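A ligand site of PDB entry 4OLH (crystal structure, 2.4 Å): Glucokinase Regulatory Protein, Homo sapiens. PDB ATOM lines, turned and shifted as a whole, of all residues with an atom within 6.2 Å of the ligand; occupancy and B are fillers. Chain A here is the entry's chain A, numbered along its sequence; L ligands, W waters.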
ATOM      1  N   THR A  43       7.157  24.044 -33.389  1.00  0.00           N
ATOM      2  CA  THR A  43       6.478  23.711 -32.154  1.00  0.00           C
ATOM      3  C   THR A  43       7.439  23.175 -31.127  1.00  0.00           C
ATOM      4  O   THR A  43       7.193  23.269 -29.918  1.00  0.00           O
ATOM      5  CB  THR A  43       5.307  22.730 -32.369  1.00  0.00           C
ATOM      6  OG1 THR A  43       5.774  21.436 -32.786  1.00  0.00           O
ATOM      7  CG2 THR A  43       4.310  23.295 -33.392  1.00  0.00           C
ATOM      8  N   GLU A  44       8.575  22.703 -31.598  1.00  0.00           N
ATOM      9  CA  GLU A  44       9.577  22.098 -30.737  1.00  0.00           C
ATOM     10  C   GLU A  44      10.673  23.029 -30.316  1.00  0.00           C
ATOM     11  O   GLU A  44      11.434  22.710 -29.429  1.00  0.00           O
ATOM     12  CB  GLU A  44      10.175  20.871 -31.432  1.00  0.00           C
ATOM     13  CG  GLU A  44       9.054  19.974 -31.970  1.00  0.00           C
ATOM     14  CD  GLU A  44       8.042  19.617 -30.914  1.00  0.00           C
ATOM     15  OE1 GLU A  44       8.482  19.057 -29.861  1.00  0.00           O
ATOM     16  OE2 GLU A  44       6.831  19.917 -31.126  1.00  0.00           O
ATOM     17  N   GLY A 119      -4.679  13.743 -28.584  1.00  0.00           N
ATOM     18  CA  GLY A 119      -4.100  13.163 -27.366  1.00  0.00           C
ATOM     19  C   GLY A 119      -3.816  14.290 -26.428  1.00  0.00           C
ATOM     20  O   GLY A 119      -3.639  15.416 -26.904  1.00  0.00           O
ATOM     21  N   GLY A 120      -3.769  14.024 -25.110  1.00  0.00           N
ATOM     22  CA  GLY A 120      -3.360  15.047 -24.099  1.00  0.00           C
ATOM     23  C   GLY A 120      -4.240  16.290 -24.213  1.00  0.00           C
ATOM     24  O   GLY A 120      -5.485  16.166 -24.410  1.00  0.00           O
ATOM     25  N   THR A 121      -3.642  17.482 -24.172  1.00  0.00           N
ATOM     26  CA  THR A 121      -4.450  18.683 -24.220  1.00  0.00           C
ATOM     27  C   THR A 121      -5.224  18.885 -25.520  1.00  0.00           C
ATOM     28  O   THR A 121      -6.294  19.505 -25.521  1.00  0.00           O
ATOM     29  CB  THR A 121      -3.628  19.917 -23.962  1.00  0.00           C
ATOM     30  OG1 THR A 121      -2.915  19.759 -22.740  1.00  0.00           O
ATOM     31  CG2 THR A 121      -4.555  21.115 -23.852  1.00  0.00           C
ATOM     32  N   SER A 122      -4.738  18.386 -26.634  1.00  0.00           N
ATOM     33  CA  SER A 122      -5.553  18.476 -27.831  1.00  0.00           C
ATOM     34  C   SER A 122      -6.822  17.722 -27.561  1.00  0.00           C
ATOM     35  O   SER A 122      -7.889  18.142 -27.986  1.00  0.00           O
ATOM     36  CB  SER A 122      -4.822  17.855 -29.008  1.00  0.00           C
ATOM     37  OG  SER A 122      -3.623  18.563 -29.206  1.00  0.00           O
ATOM     38  N   GLY A 123      -6.697  16.595 -26.845  1.00  0.00           N
ATOM     39  CA  GLY A 123      -7.854  15.802 -26.413  1.00  0.00           C
ATOM     40  C   GLY A 123      -8.797  16.514 -25.425  1.00  0.00           C
ATOM     41  O   GLY A 123     -10.014  16.490 -25.584  1.00  0.00           O
ATOM     42  N   ARG A 124      -8.220  17.137 -24.405  1.00  0.00           N
ATOM     43  CA  ARG A 124      -8.976  17.952 -23.525  1.00  0.00           C
ATOM     44  C   ARG A 124      -9.735  19.082 -24.250  1.00  0.00           C
ATOM     45  O   ARG A 124     -10.944  19.348 -23.970  1.00  0.00           O
ATOM     46  CB  ARG A 124      -8.035  18.535 -22.498  1.00  0.00           C
ATOM     47  CG  ARG A 124      -7.469  17.498 -21.576  1.00  0.00           C
ATOM     48  CD  ARG A 124      -6.770  18.141 -20.407  1.00  0.00           C
ATOM     49  NE  ARG A 124      -5.388  17.684 -20.259  1.00  0.00           N
ATOM     50  CZ  ARG A 124      -5.026  16.422 -19.977  1.00  0.00           C
ATOM     51  NH1 ARG A 124      -5.940  15.479 -19.814  1.00  0.00           N
ATOM     52  NH2 ARG A 124      -3.750  16.110 -19.864  1.00  0.00           N
ATOM     53  N   GLU A 162       0.121  10.496 -20.459  1.00  0.00           N
ATOM     54  CA  GLU A 162       0.950  10.815 -21.634  1.00  0.00           C
ATOM     55  C   GLU A 162       1.256   9.577 -22.540  1.00  0.00           C
ATOM     56  O   GLU A 162       1.468   9.751 -23.728  1.00  0.00           O
ATOM     57  CB  GLU A 162       2.248  11.496 -21.216  1.00  0.00           C
ATOM     58  CG  GLU A 162       2.088  12.848 -20.530  1.00  0.00           C
ATOM     59  CD  GLU A 162       1.725  13.973 -21.495  1.00  0.00           C
ATOM     60  OE1 GLU A 162       2.565  14.901 -21.708  1.00  0.00           O
ATOM     61  OE2 GLU A 162       0.575  13.914 -22.009  1.00  0.00           O
ATOM     62  N   GLU A 165      -0.940   8.074 -26.532  1.00  0.00           N
ATOM     63  CA  GLU A 165      -1.016   8.671 -27.878  1.00  0.00           C
ATOM     64  C   GLU A 165      -0.164   7.954 -28.962  1.00  0.00           C
ATOM     65  O   GLU A 165      -0.206   8.383 -30.138  1.00  0.00           O
ATOM     66  CB  GLU A 165      -0.620  10.144 -27.792  1.00  0.00           C
ATOM     67  CG  GLU A 165       0.817  10.412 -27.360  1.00  0.00           C
ATOM     68  CD  GLU A 165       1.219  11.896 -27.444  1.00  0.00           C
ATOM     69  OE1 GLU A 165       0.699  12.618 -26.586  1.00  0.00           O
ATOM     70  OE2 GLU A 165       2.056  12.333 -28.343  1.00  0.00           O
ATOM     71  N   ILE A 190      -6.626  16.687 -34.047  1.00  0.00           N
ATOM     72  CA  ILE A 190      -5.848  17.757 -33.486  1.00  0.00           C
ATOM     73  C   ILE A 190      -4.542  17.242 -32.933  1.00  0.00           C
ATOM     74  O   ILE A 190      -4.528  16.418 -32.019  1.00  0.00           O
ATOM     75  CB  ILE A 190      -6.631  18.454 -32.344  1.00  0.00           C
ATOM     76  CG1 ILE A 190      -7.987  18.946 -32.874  1.00  0.00           C
ATOM     77  CG2 ILE A 190      -5.809  19.577 -31.722  1.00  0.00           C
ATOM     78  CD1 ILE A 190      -8.991  19.211 -31.767  1.00  0.00           C
ATOM     79  N   SER A 191      -3.432  17.749 -33.467  1.00  0.00           N
ATOM     80  CA  SER A 191      -2.092  17.418 -32.977  1.00  0.00           C
ATOM     81  C   SER A 191      -1.175  18.590 -33.198  1.00  0.00           C
ATOM     82  O   SER A 191      -0.777  18.874 -34.309  1.00  0.00           O
ATOM     83  CB  SER A 191      -1.522  16.165 -33.653  1.00  0.00           C
ATOM     84  OG  SER A 191      -0.242  15.839 -33.098  1.00  0.00           O
ATOM     85  N   VAL A 192      -0.900  19.317 -32.128  1.00  0.00           N
ATOM     86  CA  VAL A 192      -0.246  20.559 -32.224  1.00  0.00           C
ATOM     87  C   VAL A 192       1.022  20.426 -32.989  1.00  0.00           C
ATOM     88  O   VAL A 192       1.286  21.187 -33.899  1.00  0.00           O
ATOM     89  CB  VAL A 192       0.020  21.099 -30.847  1.00  0.00           C
ATOM     90  CG1 VAL A 192       1.027  22.242 -30.908  1.00  0.00           C
ATOM     91  CG2 VAL A 192      -1.303  21.612 -30.241  1.00  0.00           C
ATOM     92  N   GLY A 193       1.827  19.429 -32.623  1.00  0.00           N
ATOM     93  CA  GLY A 193       3.075  19.211 -33.247  1.00  0.00           C
ATOM     94  C   GLY A 193       2.954  18.470 -34.563  1.00  0.00           C
ATOM     95  O   GLY A 193       3.942  18.295 -35.224  1.00  0.00           O
ATOM     96  N   LEU A 194       1.738  18.100 -34.968  1.00  0.00           N
ATOM     97  CA  LEU A 194       1.518  17.208 -36.143  1.00  0.00           C
ATOM     98  C   LEU A 194       2.398  15.940 -35.901  1.00  0.00           C
ATOM     99  O   LEU A 194       3.313  15.599 -36.633  1.00  0.00           O
ATOM    100  CB  LEU A 194       1.839  17.902 -37.452  1.00  0.00           C
ATOM    101  CG  LEU A 194       1.083  19.165 -37.886  1.00  0.00           C
ATOM    102  CD1 LEU A 194       1.439  19.538 -39.323  1.00  0.00           C
ATOM    103  CD2 LEU A 194      -0.434  19.064 -37.795  1.00  0.00           C
ATOM    104  N   SER A 195       2.089  15.299 -34.791  1.00  0.00           N
ATOM    105  CA  SER A 195       2.980  14.378 -34.139  1.00  0.00           C
ATOM    106  C   SER A 195       2.346  13.073 -33.663  1.00  0.00           C
ATOM    107  O   SER A 195       3.046  12.091 -33.580  1.00  0.00           O
ATOM    108  CB  SER A 195       3.527  15.082 -32.902  1.00  0.00           C
ATOM    109  OG  SER A 195       4.157  14.162 -32.024  1.00  0.00           O
ATOM    110  N   ALA A 196       1.070  13.085 -33.260  1.00  0.00           N
ATOM    111  CA  ALA A 196       0.509  11.999 -32.444  1.00  0.00           C
ATOM    112  C   ALA A 196       0.095  10.821 -33.326  1.00  0.00           C
ATOM    113  O   ALA A 196      -0.741  10.996 -34.206  1.00  0.00           O
ATOM    114  CB  ALA A 196      -0.650  12.478 -31.592  1.00  0.00           C
ATOM    115  N   VAL A 199      -3.644  10.327 -33.853  1.00  0.00           N
ATOM    116  CA  VAL A 199      -4.362  11.103 -34.890  1.00  0.00           C
ATOM    117  C   VAL A 199      -3.991  10.610 -36.266  1.00  0.00           C
ATOM    118  O   VAL A 199      -4.830  10.482 -37.157  1.00  0.00           O
ATOM    119  CB  VAL A 199      -4.066  12.624 -34.723  1.00  0.00           C
ATOM    120  CG1 VAL A 199      -4.720  13.475 -35.817  1.00  0.00           C
ATOM    121  CG2 VAL A 199      -4.541  13.120 -33.337  1.00  0.00           C
ATOM    122  N   GLY A 268       8.261  23.015 -26.121  1.00  0.00           N
ATOM    123  CA  GLY A 268       7.484  21.820 -26.289  1.00  0.00           C
ATOM    124  C   GLY A 268       6.281  21.797 -25.387  1.00  0.00           C
ATOM    125  O   GLY A 268       5.562  20.815 -25.344  1.00  0.00           O
ATOM    126  N   SER A 269       6.015  22.865 -24.646  1.00  0.00           N
ATOM    127  CA  SER A 269       4.837  22.794 -23.790  1.00  0.00           C
ATOM    128  C   SER A 269       3.557  23.135 -24.552  1.00  0.00           C
ATOM    129  O   SER A 269       2.906  24.137 -24.288  1.00  0.00           O
ATOM    130  CB  SER A 269       5.016  23.645 -22.540  1.00  0.00           C
ATOM    131  OG  SER A 269       3.959  23.360 -21.661  1.00  0.00           O
ATOM    132  N   SER A 270       3.172  22.263 -25.490  1.00  0.00           N
ATOM    133  CA  SER A 270       2.053  22.573 -26.361  1.00  0.00           C
ATOM    134  C   SER A 270       0.690  22.680 -25.613  1.00  0.00           C
ATOM    135  O   SER A 270      -0.346  22.992 -26.226  1.00  0.00           O
ATOM    136  CB  SER A 270       1.997  21.540 -27.488  1.00  0.00           C
ATOM    137  OG  SER A 270       1.626  20.255 -27.011  1.00  0.00           O
ATOM    138  N   ARG A 271       0.670  22.445 -24.303  1.00  0.00           N
ATOM    139  CA  ARG A 271      -0.578  22.615 -23.600  1.00  0.00           C
ATOM    140  C   ARG A 271      -1.026  24.084 -23.653  1.00  0.00           C
ATOM    141  O   ARG A 271      -2.226  24.380 -23.594  1.00  0.00           O
ATOM    142  CB  ARG A 271      -0.482  22.118 -22.147  1.00  0.00           C
ATOM    143  CG  ARG A 271       0.272  23.031 -21.195  1.00  0.00           C
ATOM    144  CD  ARG A 271       0.467  22.355 -19.863  1.00  0.00           C
ATOM    145  NE  ARG A 271       1.045  23.244 -18.853  1.00  0.00           N
ATOM    146  CZ  ARG A 271       0.357  23.873 -17.892  1.00  0.00           C
ATOM    147  NH1 ARG A 271      -0.968  23.729 -17.799  1.00  0.00           N
ATOM    148  NH2 ARG A 271       0.981  24.658 -17.025  1.00  0.00           N
ATOM    149  N   MET A 272      -0.065  24.979 -23.795  1.00  0.00           N
ATOM    150  CA  MET A 272      -0.248  26.417 -23.689  1.00  0.00           C
ATOM    151  C   MET A 272      -0.708  27.060 -24.980  1.00  0.00           C
ATOM    152  O   MET A 272      -1.904  27.020 -25.293  1.00  0.00           O
ATOM    153  CB  MET A 272       1.072  27.053 -23.204  1.00  0.00           C
ATOM    154  CG  MET A 272       1.455  26.543 -21.824  1.00  0.00           C
ATOM    155  SD  MET A 272       3.019  27.158 -21.197  1.00  0.00           S
ATOM    156  CE  MET A 272       2.372  28.577 -20.304  1.00  0.00           C
ATOM    157  N   GLU A 360      -2.451  18.890 -15.703  1.00  0.00           N
ATOM    158  CA  GLU A 360      -1.323  19.080 -16.594  1.00  0.00           C
ATOM    159  C   GLU A 360      -0.040  19.387 -15.854  1.00  0.00           C
ATOM    160  O   GLU A 360       1.051  19.057 -16.352  1.00  0.00           O
ATOM    161  CB  GLU A 360      -1.628  20.163 -17.630  1.00  0.00           C
ATOM    162  CG  GLU A 360      -2.606  19.629 -18.689  1.00  0.00           C
ATOM    163  CD  GLU A 360      -3.352  20.681 -19.490  1.00  0.00           C
ATOM    164  OE1 GLU A 360      -3.204  21.911 -19.245  1.00  0.00           O
ATOM    165  OE2 GLU A 360      -4.122  20.242 -20.377  1.00  0.00           O
ATOM    166  N   HIS A 363       2.423  15.941 -15.344  1.00  0.00           N
ATOM    167  CA  HIS A 363       3.415  15.505 -16.322  1.00  0.00           C
ATOM    168  C   HIS A 363       4.374  16.595 -16.680  1.00  0.00           C
ATOM    169  O   HIS A 363       5.556  16.359 -16.778  1.00  0.00           O
ATOM    170  CB  HIS A 363       2.821  14.907 -17.594  1.00  0.00           C
ATOM    171  CG  HIS A 363       1.654  15.664 -18.162  1.00  0.00           C
ATOM    172  ND1 HIS A 363       0.396  15.117 -18.249  1.00  0.00           N
ATOM    173  CD2 HIS A 363       1.575  16.891 -18.718  1.00  0.00           C
ATOM    174  CE1 HIS A 363      -0.413  15.984 -18.806  1.00  0.00           C
ATOM    175  NE2 HIS A 363       0.272  17.074 -19.103  1.00  0.00           N
ATOM    176  N   THR A 364       3.873  17.806 -16.836  1.00  0.00           N
ATOM    177  CA  THR A 364       4.709  18.891 -17.272  1.00  0.00           C
ATOM    178  C   THR A 364       5.810  19.187 -16.267  1.00  0.00           C
ATOM    179  O   THR A 364       6.968  19.412 -16.657  1.00  0.00           O
ATOM    180  CB  THR A 364       3.880  20.153 -17.508  1.00  0.00           C
ATOM    181  OG1 THR A 364       2.877  19.863 -18.487  1.00  0.00           O
ATOM    182  CG2 THR A 364       4.760  21.333 -17.954  1.00  0.00           C
ATOM    183  N   ASN A 524       6.350   8.901 -23.255  1.00  0.00           N
ATOM    184  CA  ASN A 524       5.973   8.507 -24.611  1.00  0.00           C
ATOM    185  C   ASN A 524       7.166   8.758 -25.545  1.00  0.00           C
ATOM    186  O   ASN A 524       8.168   9.362 -25.096  1.00  0.00           O
ATOM    187  CB  ASN A 524       4.683   9.215 -25.092  1.00  0.00           C
ATOM    188  CG  ASN A 524       4.752  10.728 -24.987  1.00  0.00           C
ATOM    189  OD1 ASN A 524       3.825  11.367 -24.566  1.00  0.00           O
ATOM    190  ND2 ASN A 524       5.840  11.292 -25.424  1.00  0.00           N
ATOM    191  N   LYS A 526       7.716  10.832 -28.045  1.00  0.00           N
ATOM    192  CA  LYS A 526       8.029  12.242 -28.302  1.00  0.00           C
ATOM    193  C   LYS A 526       8.907  12.838 -27.191  1.00  0.00           C
ATOM    194  O   LYS A 526       9.923  13.516 -27.446  1.00  0.00           O
ATOM    195  CB  LYS A 526       6.744  13.045 -28.529  1.00  0.00           C
ATOM    196  CG  LYS A 526       6.931  14.555 -28.559  1.00  0.00           C
ATOM    197  CD  LYS A 526       5.601  15.254 -28.853  1.00  0.00           C
ATOM    198  CE  LYS A 526       4.699  15.290 -27.625  1.00  0.00           C
ATOM    199  NZ  LYS A 526       3.391  15.899 -27.952  1.00  0.00           N
HETATM  200  C1  LIG L   1       2.063  19.279 -23.855  1.00  0.00           C
HETATM  201  C2  LIG L   1       1.096  18.298 -23.243  1.00  0.00           C
HETATM  202  C3  LIG L   1       0.974  17.047 -24.047  1.00  0.00           C
HETATM  203  C4  LIG L   1       0.278  17.234 -25.381  1.00  0.00           C
HETATM  204  C5  LIG L   1       0.076  15.887 -26.037  1.00  0.00           C
HETATM  205  C6  LIG L   1      -0.273  16.011 -27.523  1.00  0.00           C
HETATM  206  O1  LIG L   1       2.085  20.413 -22.960  1.00  0.00           O
HETATM  207  O2  LIG L   1       1.554  17.972 -21.927  1.00  0.00           O
HETATM  208  O3  LIG L   1       0.189  16.111 -23.308  1.00  0.00           O
HETATM  209  O4  LIG L   1      -0.998  17.858 -25.199  1.00  0.00           O
HETATM  210  O5  LIG L   1       1.260  15.090 -25.922  1.00  0.00           O
HETATM  211  O6  LIG L   1       0.581  16.927 -28.204  1.00  0.00           O
HETATM  212  P1  LIG L   1       0.237  17.108 -29.747  1.00  0.00           P
HETATM  213  O7  LIG L   1       1.438  17.824 -30.351  1.00  0.00           O
HETATM  214  O8  LIG L   1      -0.148  15.709 -30.509  1.00  0.00           O
HETATM  215  O9  LIG L   1      -1.162  17.883 -29.730  1.00  0.00           O
HETATM  216  O   HOH W   1       2.173  14.434 -29.947  1.00  0.00           O
HETATM  217  O   HOH W   2      -2.826  14.716 -30.604  1.00  0.00           O
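Water W1 lies within hydrogen-bond range of the side-chain carboxylate (OE2) of Glu 165, an oxygen (O8) of the ligand, the side-chain amino group (NZ) of Lys 526 and the side-chain hydroxyl (OG) of Ser 195.
Water W2 lies within hydrogen-bond range of O of Ile 190 (2.8 Å), O8 of the ligand (2.9 Å) and N of Gly 119 (2.9 Å).
Residues that only touch the ligand: Gly 119, Gly 120, Ala 196 and Ser 269.
Within 4 Å of the ligand: Gly 119, Gly 120, Thr 121, Ser 122, Glu 162, Glu 165, Ser 191, Val 192, Gly 193, Ala 196, Ser 269, Ser 270, Arg 271, His 363 and Lys 526.
The nearest printed residue that does not touch the ligand is Gly 268 (4.1 Å).
The side-chain amide oxygen of Asn 524 sits close to the backbone carbonyl oxygen of Glu 162, 3.0 Å away.
OG of Ser 191 lies within hydrogen-bond range of N of Ala 196.
The backbone NH (N) of Ser 195 sits at hydrogen-bond distance from the side-chain hydroxyl (OG) of Ser 191, 2.9 Å away.
OE2 of Glu 165 is in salt-bridge range of NZ of Lys 526 (3.8 Å).
NH1 of Arg 271 lies within salt-bridge range of OE1 of Glu 360 (3.2 Å).
OE2 of Glu 360 sits at hydrogen-bond distance from OG1 of Thr 121.
N of Lys 526 lies close to ND2 of Asn 524, 3.3 Å away.
NE2 of His 363 lies close to O of Glu 360.
An oxygen (O3) of the ligand is in hydrogen-bond range of the side-chain carboxylate of Glu 162, at 2.6 Å.
An oxygen (O8) of the ligand lies within hydrogen-bond range of the side-chain hydroxyl (OG) of Ser 191 (2.6 Å).
The side-chain hydroxyl (OG) of Ser 122 is in hydrogen-bond range of an oxygen (O9) of the ligand.
O5 of the ligand lies within hydrogen-bond range of OE1 of Glu 165 (2.6 Å).
An oxygen (O9) of the ligand is in hydrogen-bond range of the backbone NH (N) of Val 192 (2.8 Å).
The backbone NH (N) of Gly 193 sits at hydrogen-bond distance from an oxygen (O7) of the ligand (2.8 Å).
O1 of the ligand lies within hydrogen-bond range of N of Arg 271 (2.8 Å).
An oxygen (O4) of the ligand sits at hydrogen-bond distance from the backbone NH of Thr 121 (2.9 Å).
The side-chain amino group (NZ) of Lys 526 is in salt-bridge range of an oxygen (O7) of the ligand, at 3.6 Å.
An oxygen (O2) of the ligand sits at hydrogen-bond distance from a ring nitrogen (NE2) of His 363, at 3.2 Å.
The backbone NH (N) of Ser 270 lies within hydrogen-bond range of an oxygen (O1) of the ligand, 3.3 Å away.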
